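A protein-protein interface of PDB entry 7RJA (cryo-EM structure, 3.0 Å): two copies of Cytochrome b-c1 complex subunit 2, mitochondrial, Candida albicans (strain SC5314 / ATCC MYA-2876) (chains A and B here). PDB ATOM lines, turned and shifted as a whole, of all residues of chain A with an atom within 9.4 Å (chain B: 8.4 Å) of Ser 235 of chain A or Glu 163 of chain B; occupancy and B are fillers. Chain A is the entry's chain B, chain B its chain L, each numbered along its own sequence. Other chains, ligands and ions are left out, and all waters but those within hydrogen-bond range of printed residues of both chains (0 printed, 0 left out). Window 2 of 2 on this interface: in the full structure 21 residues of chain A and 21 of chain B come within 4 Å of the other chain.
Pro 233 of chain A touches Ser 164 of chain B (CB to OG, 3.96 Å). O of Ser 234 of chain A touches CB of Ser 164 of chain B, at 3.2 Å. Ser 235 of chain A touches Glu 163 of chain B. O of Gly 363 of chain A touches CB of Ser 164 of chain B, 3.5 Å away.
Of the printed residues of chain B, Pro 233 of chain A touches Ser 164 (3.96 Å). Ser 235 of chain A touches just one residue of chain B: Glu 163 (3.8 Å). No residue of chain B comes within 4 Å of Gly 236 of chain A. Printed residues of chain B within 4 Å of Gly 363 of chain A: Ser 164. Printed residues of chain B within 4 Å of Asp 364 of chain A: Ser 164 and Thr 165. No residue of chain A comes within 4 Å of Asn 162 of chain B. Ser 164 of chain B touches four residues of chain A. Of the printed residues of chain A, Thr 165 of chain B touches Asp 364 (2.5 Å). The nearest residue of chain B that does not touch Ser 235 of chain A is Ser 164 of chain B (4.2 Å). The nearest residue of chain A that does not touch Glu 163 of chain B is Ser 234 of chain A (5.4 Å).
The side-chain amino group of Lys 141 of chain A sits at hydrogen-bond distance from the side-chain hydroxyl of Ser 234 of chain A. The backbone carbonyl oxygen of Val 232 of chain A lies within hydrogen-bond range of the backbone NH of Gly 363 of chain A, at 3.5 Å. The backbone NH (N) of Ser 234 of chain A lies within hydrogen-bond range of the backbone carbonyl oxygen (O) of Gly 363 of chain A, 3.5 Å away. OG of Ser 238 of chain A is in hydrogen-bond range of N of Asp 364 of chain A (3.1 Å). OD1 of Asn 162 of chain B lies close to OE2 of Glu 163 of chain B, 2.8 Å away. N of Ser 164 of chain B lies within hydrogen-bond range of OD1 of Asn 162 of chain B (2.8 Å).
Printed residues of chain B that touch a printed residue of chain A: Glu 163, Ser 164 and Thr 165. Hydrophobic or aromatic side chains of chain A that line the printed part of chain B: Pro 233. Among the printed residues, 6 pairs touch across the chains.
The side-chain carboxylate (OD1) of Asp 364 of chain A lies within hydrogen-bond range of the side-chain hydroxyl (OG1) of Thr 165 of chain B (2.5 Å). OD1 of Asp 364 of chain A sits close to O of Ser 164 of chain B, 3.3 Å away.
Position printed for both chains: 135. Of the 6 pairs that touch across the chains among the printed residues, none has its exchanged pair printed and touching as well.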
ATOM      1  N   ASN A 135       7.102  13.878 -31.602  1.00  0.00           N
ATOM      2  CA  ASN A 135       8.322  13.691 -30.827  1.00  0.00           C
ATOM      3  C   ASN A 135       9.411  12.986 -31.620  1.00  0.00           C
ATOM      4  O   ASN A 135      10.587  13.111 -31.272  1.00  0.00           O
ATOM      5  CB  ASN A 135       8.022  12.909 -29.552  1.00  0.00           C
ATOM      6  CG  ASN A 135       7.303  13.743 -28.518  1.00  0.00           C
ATOM      7  OD1 ASN A 135       7.124  14.946 -28.692  1.00  0.00           O
ATOM      8  ND2 ASN A 135       6.892  13.108 -27.428  1.00  0.00           N
ATOM      9  N   ALA A 136       9.055  12.256 -32.676  1.00  0.00           N
ATOM     10  CA  ALA A 136      10.081  11.656 -33.519  1.00  0.00           C
ATOM     11  C   ALA A 136      11.016  12.717 -34.076  1.00  0.00           C
ATOM     12  O   ALA A 136      12.171  12.421 -34.398  1.00  0.00           O
ATOM     13  CB  ALA A 136       9.438  10.864 -34.655  1.00  0.00           C
ATOM     14  N   ASN A 137      10.535  13.951 -34.195  1.00  0.00           N
ATOM     15  CA  ASN A 137      11.353  15.073 -34.622  1.00  0.00           C
ATOM     16  C   ASN A 137      12.163  15.557 -33.426  1.00  0.00           C
ATOM     17  O   ASN A 137      11.583  16.044 -32.450  1.00  0.00           O
ATOM     18  CB  ASN A 137      10.470  16.193 -35.171  1.00  0.00           C
ATOM     19  CG  ASN A 137      11.258  17.420 -35.574  1.00  0.00           C
ATOM     20  OD1 ASN A 137      12.462  17.507 -35.345  1.00  0.00           O
ATOM     21  ND2 ASN A 137      10.573  18.388 -36.171  1.00  0.00           N
ATOM     22  N   PRO A 138      13.492  15.445 -33.450  1.00  0.00           N
ATOM     23  CA  PRO A 138      14.266  15.865 -32.275  1.00  0.00           C
ATOM     24  C   PRO A 138      14.098  17.331 -31.944  1.00  0.00           C
ATOM     25  O   PRO A 138      14.147  17.699 -30.764  1.00  0.00           O
ATOM     26  CB  PRO A 138      15.706  15.530 -32.675  1.00  0.00           C
ATOM     27  CG  PRO A 138      15.701  15.619 -34.146  1.00  0.00           C
ATOM     28  CD  PRO A 138      14.373  15.076 -34.570  1.00  0.00           C
ATOM     29  N   ALA A 139      13.896  18.186 -32.946  1.00  0.00           N
ATOM     30  CA  ALA A 139      13.718  19.606 -32.670  1.00  0.00           C
ATOM     31  C   ALA A 139      12.471  19.862 -31.838  1.00  0.00           C
ATOM     32  O   ALA A 139      12.503  20.672 -30.906  1.00  0.00           O
ATOM     33  CB  ALA A 139      13.648  20.389 -33.977  1.00  0.00           C
ATOM     34  N   LYS A 141      10.854  17.705 -29.815  1.00  0.00           N
ATOM     35  CA  LYS A 141      11.082  17.187 -28.472  1.00  0.00           C
ATOM     36  C   LYS A 141      11.942  18.148 -27.669  1.00  0.00           C
ATOM     37  O   LYS A 141      11.663  18.421 -26.494  1.00  0.00           O
ATOM     38  CB  LYS A 141      11.750  15.817 -28.554  1.00  0.00           C
ATOM     39  CG  LYS A 141      11.784  15.066 -27.240  1.00  0.00           C
ATOM     40  CD  LYS A 141      12.573  13.772 -27.354  1.00  0.00           C
ATOM     41  CE  LYS A 141      12.009  12.854 -28.417  1.00  0.00           C
ATOM     42  NZ  LYS A 141      12.599  11.496 -28.335  1.00  0.00           N
ATOM     43  N   VAL A 232      17.857  14.992 -23.244  1.00  0.00           N
ATOM     44  CA  VAL A 232      16.839  13.993 -23.547  1.00  0.00           C
ATOM     45  C   VAL A 232      17.405  13.012 -24.566  1.00  0.00           C
ATOM     46  O   VAL A 232      17.344  13.285 -25.770  1.00  0.00           O
ATOM     47  CB  VAL A 232      15.558  14.647 -24.084  1.00  0.00           C
ATOM     48  CG1 VAL A 232      14.480  13.605 -24.282  1.00  0.00           C
ATOM     49  CG2 VAL A 232      15.082  15.744 -23.152  1.00  0.00           C
ATOM     50  N   PRO A 233      17.955  11.872 -24.153  1.00  0.00           N
ATOM     51  CA  PRO A 233      18.534  10.954 -25.137  1.00  0.00           C
ATOM     52  C   PRO A 233      17.491  10.501 -26.145  1.00  0.00           C
ATOM     53  O   PRO A 233      16.334  10.255 -25.801  1.00  0.00           O
ATOM     54  CB  PRO A 233      19.042   9.789 -24.282  1.00  0.00           C
ATOM     55  CG  PRO A 233      18.215   9.836 -23.059  1.00  0.00           C
ATOM     56  CD  PRO A 233      17.934  11.282 -22.805  1.00  0.00           C
ATOM     57  N   SER A 234      17.913  10.395 -27.401  1.00  0.00           N
ATOM     58  CA  SER A 234      17.011  10.029 -28.480  1.00  0.00           C
ATOM     59  C   SER A 234      17.808   9.371 -29.595  1.00  0.00           C
ATOM     60  O   SER A 234      19.010   9.603 -29.738  1.00  0.00           O
ATOM     61  CB  SER A 234      16.259  11.251 -29.019  1.00  0.00           C
ATOM     62  OG  SER A 234      15.275  10.870 -29.964  1.00  0.00           O
ATOM     63  N   SER A 235      17.124   8.545 -30.378  1.00  0.00           N
ATOM     64  CA  SER A 235      17.750   7.875 -31.504  1.00  0.00           C
ATOM     65  C   SER A 235      17.701   8.761 -32.744  1.00  0.00           C
ATOM     66  O   SER A 235      17.024   9.791 -32.785  1.00  0.00           O
ATOM     67  CB  SER A 235      17.061   6.542 -31.781  1.00  0.00           C
ATOM     68  OG  SER A 235      17.323   5.608 -30.750  1.00  0.00           O
ATOM     69  N   GLY A 236      18.436   8.344 -33.771  1.00  0.00           N
ATOM     70  CA  GLY A 236      18.404   9.070 -35.027  1.00  0.00           C
ATOM     71  C   GLY A 236      18.994  10.460 -34.896  1.00  0.00           C
ATOM     72  O   GLY A 236      20.043  10.666 -34.277  1.00  0.00           O
ATOM     73  N   ALA A 237      18.310  11.432 -35.492  1.00  0.00           N
ATOM     74  CA  ALA A 237      18.833  12.788 -35.551  1.00  0.00           C
ATOM     75  C   ALA A 237      18.933  13.396 -34.159  1.00  0.00           C
ATOM     76  O   ALA A 237      18.092  13.150 -33.292  1.00  0.00           O
ATOM     77  CB  ALA A 237      17.940  13.655 -36.438  1.00  0.00           C
ATOM     78  N   SER A 238      19.974  14.194 -33.952  1.00  0.00           N
ATOM     79  CA  SER A 238      20.182  14.923 -32.713  1.00  0.00           C
ATOM     80  C   SER A 238      19.811  16.386 -32.903  1.00  0.00           C
ATOM     81  O   SER A 238      19.573  16.854 -34.017  1.00  0.00           O
ATOM     82  CB  SER A 238      21.636  14.801 -32.255  1.00  0.00           C
ATOM     83  OG  SER A 238      21.992  13.447 -32.060  1.00  0.00           O
ATOM     84  N   SER A 239      19.776  17.116 -31.792  1.00  0.00           N
ATOM     85  CA  SER A 239      19.372  18.513 -31.831  1.00  0.00           C
ATOM     86  C   SER A 239      19.752  19.199 -30.527  1.00  0.00           C
ATOM     87  O   SER A 239      19.472  18.682 -29.447  1.00  0.00           O
ATOM     88  CB  SER A 239      17.864  18.638 -32.066  1.00  0.00           C
ATOM     89  OG  SER A 239      17.396  19.911 -31.667  1.00  0.00           O
ATOM     90  N   GLY A 298      20.455  17.623 -36.682  1.00  0.00           N
ATOM     91  CA  GLY A 298      21.166  16.792 -37.631  1.00  0.00           C
ATOM     92  C   GLY A 298      22.118  15.822 -36.965  1.00  0.00           C
ATOM     93  O   GLY A 298      21.847  15.332 -35.866  1.00  0.00           O
ATOM     94  N   ALA A 300      24.995  14.337 -34.768  1.00  0.00           N
ATOM     95  CA  ALA A 300      25.416  14.798 -33.451  1.00  0.00           C
ATOM     96  C   ALA A 300      26.732  15.559 -33.523  1.00  0.00           C
ATOM     97  O   ALA A 300      26.884  16.615 -32.898  1.00  0.00           O
ATOM     98  CB  ALA A 300      25.540  13.614 -32.497  1.00  0.00           C
ATOM     99  N   VAL A 362      19.416  16.772 -27.300  1.00  0.00           N
ATOM    100  CA  VAL A 362      18.666  15.575 -27.648  1.00  0.00           C
ATOM    101  C   VAL A 362      19.493  14.774 -28.637  1.00  0.00           C
ATOM    102  O   VAL A 362      20.099  15.343 -29.549  1.00  0.00           O
ATOM    103  CB  VAL A 362      17.292  15.924 -28.252  1.00  0.00           C
ATOM    104  CG1 VAL A 362      16.477  14.671 -28.477  1.00  0.00           C
ATOM    105  CG2 VAL A 362      16.552  16.897 -27.359  1.00  0.00           C
ATOM    106  N   GLY A 363      19.520  13.458 -28.461  1.00  0.00           N
ATOM    107  CA  GLY A 363      20.217  12.596 -29.393  1.00  0.00           C
ATOM    108  C   GLY A 363      21.401  11.884 -28.781  1.00  0.00           C
ATOM    109  O   GLY A 363      21.264  11.206 -27.760  1.00  0.00           O
ATOM    110  N   ASP A 364      22.570  12.024 -29.399  1.00  0.00           N
ATOM    111  CA  ASP A 364      23.786  11.362 -28.932  1.00  0.00           C
ATOM    112  C   ASP A 364      24.404  12.222 -27.841  1.00  0.00           C
ATOM    113  O   ASP A 364      25.289  13.041 -28.087  1.00  0.00           O
ATOM    114  CB  ASP A 364      24.751  11.141 -30.087  1.00  0.00           C
ATOM    115  CG  ASP A 364      25.855  10.165 -29.747  1.00  0.00           C
ATOM    116  OD1 ASP A 364      25.765   9.506 -28.691  1.00  0.00           O
ATOM    117  OD2 ASP A 364      26.809  10.045 -30.542  1.00  0.00           O
ATOM    118  N   LEU A 365      23.936  12.024 -26.608  1.00  0.00           N
ATOM    119  CA  LEU A 365      24.372  12.870 -25.504  1.00  0.00           C
ATOM    120  C   LEU A 365      25.862  12.747 -25.232  1.00  0.00           C
ATOM    121  O   LEU A 365      26.428  13.609 -24.553  1.00  0.00           O
ATOM    122  CB  LEU A 365      23.589  12.527 -24.241  1.00  0.00           C
ATOM    123  CG  LEU A 365      22.263  13.267 -24.077  1.00  0.00           C
ATOM    124  CD1 LEU A 365      21.450  13.206 -25.351  1.00  0.00           C
ATOM    125  CD2 LEU A 365      21.480  12.683 -22.920  1.00  0.00           C
ATOM    126  N   SER B  45      29.749   6.314 -24.069  1.00  0.00           N
ATOM    127  CA  SER B  45      28.585   5.808 -23.352  1.00  0.00           C
ATOM    128  C   SER B  45      28.157   4.441 -23.863  1.00  0.00           C
ATOM    129  O   SER B  45      27.781   4.289 -25.028  1.00  0.00           O
ATOM    130  CB  SER B  45      27.434   6.805 -23.492  1.00  0.00           C
ATOM    131  OG  SER B  45      27.839   8.107 -23.113  1.00  0.00           O
ATOM    132  N   GLY B  46      28.210   3.447 -22.980  1.00  0.00           N
ATOM    133  CA  GLY B  46      27.665   2.137 -23.262  1.00  0.00           C
ATOM    134  C   GLY B  46      28.631   1.119 -23.827  1.00  0.00           C
ATOM    135  O   GLY B  46      28.249  -0.045 -23.980  1.00  0.00           O
ATOM    136  N   LEU B 124      24.053  -7.134 -29.002  1.00  0.00           N
ATOM    137  CA  LEU B 124      23.107  -6.038 -29.145  1.00  0.00           C
ATOM    138  C   LEU B 124      21.717  -6.465 -28.691  1.00  0.00           C
ATOM    139  O   LEU B 124      21.066  -5.720 -27.951  1.00  0.00           O
ATOM    140  CB  LEU B 124      23.063  -5.516 -30.581  1.00  0.00           C
ATOM    141  CG  LEU B 124      24.332  -4.842 -31.093  1.00  0.00           C
ATOM    142  CD1 LEU B 124      24.177  -4.510 -32.564  1.00  0.00           C
ATOM    143  CD2 LEU B 124      24.633  -3.588 -30.293  1.00  0.00           C
ATOM    144  N   ALA B 127      22.002  -6.797 -24.876  1.00  0.00           N
ATOM    145  CA  ALA B 127      22.229  -5.500 -24.251  1.00  0.00           C
ATOM    146  C   ALA B 127      20.964  -4.656 -24.273  1.00  0.00           C
ATOM    147  O   ALA B 127      20.608  -4.034 -23.267  1.00  0.00           O
ATOM    148  CB  ALA B 127      23.369  -4.769 -24.955  1.00  0.00           C
ATOM    149  N   ASN B 128      20.272  -4.622 -25.411  1.00  0.00           N
ATOM    150  CA  ASN B 128      19.037  -3.852 -25.497  1.00  0.00           C
ATOM    151  C   ASN B 128      17.968  -4.422 -24.577  1.00  0.00           C
ATOM    152  O   ASN B 128      17.241  -3.669 -23.920  1.00  0.00           O
ATOM    153  CB  ASN B 128      18.542  -3.820 -26.941  1.00  0.00           C
ATOM    154  CG  ASN B 128      19.429  -2.984 -27.840  1.00  0.00           C
ATOM    155  OD1 ASN B 128      20.219  -2.171 -27.368  1.00  0.00           O
ATOM    156  ND2 ASN B 128      19.299  -3.179 -29.145  1.00  0.00           N
ATOM    157  N   ALA B 129      17.855  -5.750 -24.513  1.00  0.00           N
ATOM    158  CA  ALA B 129      16.867  -6.355 -23.629  1.00  0.00           C
ATOM    159  C   ALA B 129      17.143  -5.991 -22.179  1.00  0.00           C
ATOM    160  O   ALA B 129      16.227  -5.630 -21.433  1.00  0.00           O
ATOM    161  CB  ALA B 129      16.863  -7.872 -23.810  1.00  0.00           C
ATOM    162  N   THR B 131      18.864  -3.398 -21.040  1.00  0.00           N
ATOM    163  CA  THR B 131      18.624  -1.974 -20.843  1.00  0.00           C
ATOM    164  C   THR B 131      17.140  -1.696 -20.669  1.00  0.00           C
ATOM    165  O   THR B 131      16.737  -0.951 -19.770  1.00  0.00           O
ATOM    166  CB  THR B 131      19.177  -1.180 -22.024  1.00  0.00           C
ATOM    167  OG1 THR B 131      20.605  -1.262 -22.034  1.00  0.00           O
ATOM    168  CG2 THR B 131      18.760   0.274 -21.929  1.00  0.00           C
ATOM    169  N   LYS B 132      16.308  -2.293 -21.521  1.00  0.00           N
ATOM    170  CA  LYS B 132      14.870  -2.076 -21.420  1.00  0.00           C
ATOM    171  C   LYS B 132      14.331  -2.618 -20.103  1.00  0.00           C
ATOM    172  O   LYS B 132      13.496  -1.982 -19.451  1.00  0.00           O
ATOM    173  CB  LYS B 132      14.160  -2.729 -22.604  1.00  0.00           C
ATOM    174  CG  LYS B 132      12.666  -2.482 -22.634  1.00  0.00           C
ATOM    175  CD  LYS B 132      12.022  -3.106 -23.857  1.00  0.00           C
ATOM    176  CE  LYS B 132      10.543  -2.776 -23.926  1.00  0.00           C
ATOM    177  NZ  LYS B 132       9.778  -3.426 -22.827  1.00  0.00           N
ATOM    178  N   ASN B 135      15.627  -0.179 -17.198  1.00  0.00           N
ATOM    179  CA  ASN B 135      14.989   1.130 -17.232  1.00  0.00           C
ATOM    180  C   ASN B 135      13.501   1.055 -16.931  1.00  0.00           C
ATOM    181  O   ASN B 135      12.900   2.077 -16.588  1.00  0.00           O
ATOM    182  CB  ASN B 135      15.206   1.784 -18.593  1.00  0.00           C
ATOM    183  CG  ASN B 135      16.631   2.239 -18.795  1.00  0.00           C
ATOM    184  OD1 ASN B 135      17.442   2.197 -17.873  1.00  0.00           O
ATOM    185  ND2 ASN B 135      16.946   2.677 -20.005  1.00  0.00           N
ATOM    186  N   PHE B 160      24.346   1.316 -19.058  1.00  0.00           N
ATOM    187  CA  PHE B 160      23.991   0.335 -20.069  1.00  0.00           C
ATOM    188  C   PHE B 160      23.974   0.970 -21.451  1.00  0.00           C
ATOM    189  O   PHE B 160      23.834   2.186 -21.604  1.00  0.00           O
ATOM    190  CB  PHE B 160      22.619  -0.287 -19.786  1.00  0.00           C
ATOM    191  CG  PHE B 160      22.542  -1.030 -18.487  1.00  0.00           C
ATOM    192  CD1 PHE B 160      23.615  -1.769 -18.029  1.00  0.00           C
ATOM    193  CD2 PHE B 160      21.389  -1.001 -17.733  1.00  0.00           C
ATOM    194  CE1 PHE B 160      23.539  -2.455 -16.843  1.00  0.00           C
ATOM    195  CE2 PHE B 160      21.310  -1.686 -16.548  1.00  0.00           C
ATOM    196  CZ  PHE B 160      22.386  -2.413 -16.101  1.00  0.00           C
ATOM    197  N   TYR B 161      24.111   0.118 -22.462  1.00  0.00           N
ATOM    198  CA  TYR B 161      24.112   0.575 -23.841  1.00  0.00           C
ATOM    199  C   TYR B 161      22.746   1.125 -24.225  1.00  0.00           C
ATOM    200  O   TYR B 161      21.709   0.548 -23.891  1.00  0.00           O
ATOM    201  CB  TYR B 161      24.490  -0.574 -24.771  1.00  0.00           C
ATOM    202  CG  TYR B 161      24.296  -0.274 -26.235  1.00  0.00           C
ATOM    203  CD1 TYR B 161      25.141   0.594 -26.904  1.00  0.00           C
ATOM    204  CD2 TYR B 161      23.270  -0.866 -26.951  1.00  0.00           C
ATOM    205  CE1 TYR B 161      24.968   0.865 -28.240  1.00  0.00           C
ATOM    206  CE2 TYR B 161      23.090  -0.601 -28.287  1.00  0.00           C
ATOM    207  CZ  TYR B 161      23.941   0.266 -28.927  1.00  0.00           C
ATOM    208  OH  TYR B 161      23.761   0.533 -30.263  1.00  0.00           O
ATOM    209  N   ASN B 162      22.755   2.250 -24.932  1.00  0.00           N
ATOM    210  CA  ASN B 162      21.544   2.878 -25.433  1.00  0.00           C
ATOM    211  C   ASN B 162      21.739   3.191 -26.907  1.00  0.00           C
ATOM    212  O   ASN B 162      22.814   3.635 -27.317  1.00  0.00           O
ATOM    213  CB  ASN B 162      21.221   4.157 -24.658  1.00  0.00           C
ATOM    214  CG  ASN B 162      19.951   4.830 -25.138  1.00  0.00           C
ATOM    215  OD1 ASN B 162      19.520   4.638 -26.274  1.00  0.00           O
ATOM    216  ND2 ASN B 162      19.345   5.628 -24.268  1.00  0.00           N
ATOM    217  N   GLU B 163      20.693   2.967 -27.702  1.00  0.00           N
ATOM    218  CA  GLU B 163      20.815   3.171 -29.140  1.00  0.00           C
ATOM    219  C   GLU B 163      21.103   4.622 -29.487  1.00  0.00           C
ATOM    220  O   GLU B 163      21.554   4.902 -30.602  1.00  0.00           O
ATOM    221  CB  GLU B 163      19.548   2.717 -29.875  1.00  0.00           C
ATOM    222  CG  GLU B 163      18.955   1.386 -29.424  1.00  0.00           C
ATOM    223  CD  GLU B 163      18.070   1.507 -28.199  1.00  0.00           C
ATOM    224  OE1 GLU B 163      17.179   0.651 -28.021  1.00  0.00           O
ATOM    225  OE2 GLU B 163      18.265   2.460 -27.415  1.00  0.00           O
ATOM    226  N   SER B 164      20.858   5.550 -28.562  1.00  0.00           N
ATOM    227  CA  SER B 164      21.113   6.959 -28.829  1.00  0.00           C
ATOM    228  C   SER B 164      22.579   7.246 -29.104  1.00  0.00           C
ATOM    229  O   SER B 164      22.886   8.282 -29.703  1.00  0.00           O
ATOM    230  CB  SER B 164      20.642   7.807 -27.648  1.00  0.00           C
ATOM    231  OG  SER B 164      21.461   7.595 -26.514  1.00  0.00           O
ATOM    232  N   THR B 165      23.484   6.363 -28.693  1.00  0.00           N
ATOM    233  CA  THR B 165      24.922   6.527 -28.899  1.00  0.00           C
ATOM    234  C   THR B 165      25.425   5.271 -29.596  1.00  0.00           C
ATOM    235  O   THR B 165      25.973   4.367 -28.953  1.00  0.00           O
ATOM    236  CB  THR B 165      25.652   6.758 -27.576  1.00  0.00           C
ATOM    237  OG1 THR B 165      25.110   7.911 -26.923  1.00  0.00           O
ATOM    238  CG2 THR B 165      27.133   6.970 -27.816  1.00  0.00           C
ATOM    239  N   PRO B 166      25.253   5.182 -30.913  1.00  0.00           N
ATOM    240  CA  PRO B 166      25.567   3.930 -31.608  1.00  0.00           C
ATOM    241  C   PRO B 166      27.011   3.514 -31.391  1.00  0.00           C
ATOM    242  O   PRO B 166      27.922   4.343 -31.371  1.00  0.00           O
ATOM    243  CB  PRO B 166      25.293   4.264 -33.077  1.00  0.00           C
ATOM    244  CG  PRO B 166      24.362   5.414 -33.040  1.00  0.00           C
ATOM    245  CD  PRO B 166      24.751   6.208 -31.838  1.00  0.00           C
ATOM    246  N   ILE B 167      27.208   2.209 -31.229  1.00  0.00           N
ATOM    247  CA  ILE B 167      28.524   1.614 -31.042  1.00  0.00           C
ATOM    248  C   ILE B 167      28.705   0.547 -32.108  1.00  0.00           C
ATOM    249  O   ILE B 167      27.823  -0.298 -32.300  1.00  0.00           O
ATOM    250  CB  ILE B 167      28.682   1.004 -29.639  1.00  0.00           C
ATOM    251  CG1 ILE B 167      28.404   2.049 -28.558  1.00  0.00           C
ATOM    252  CG2 ILE B 167      30.070   0.428 -29.473  1.00  0.00           C
ATOM    253  CD1 ILE B 167      29.347   3.221 -28.574  1.00  0.00           C
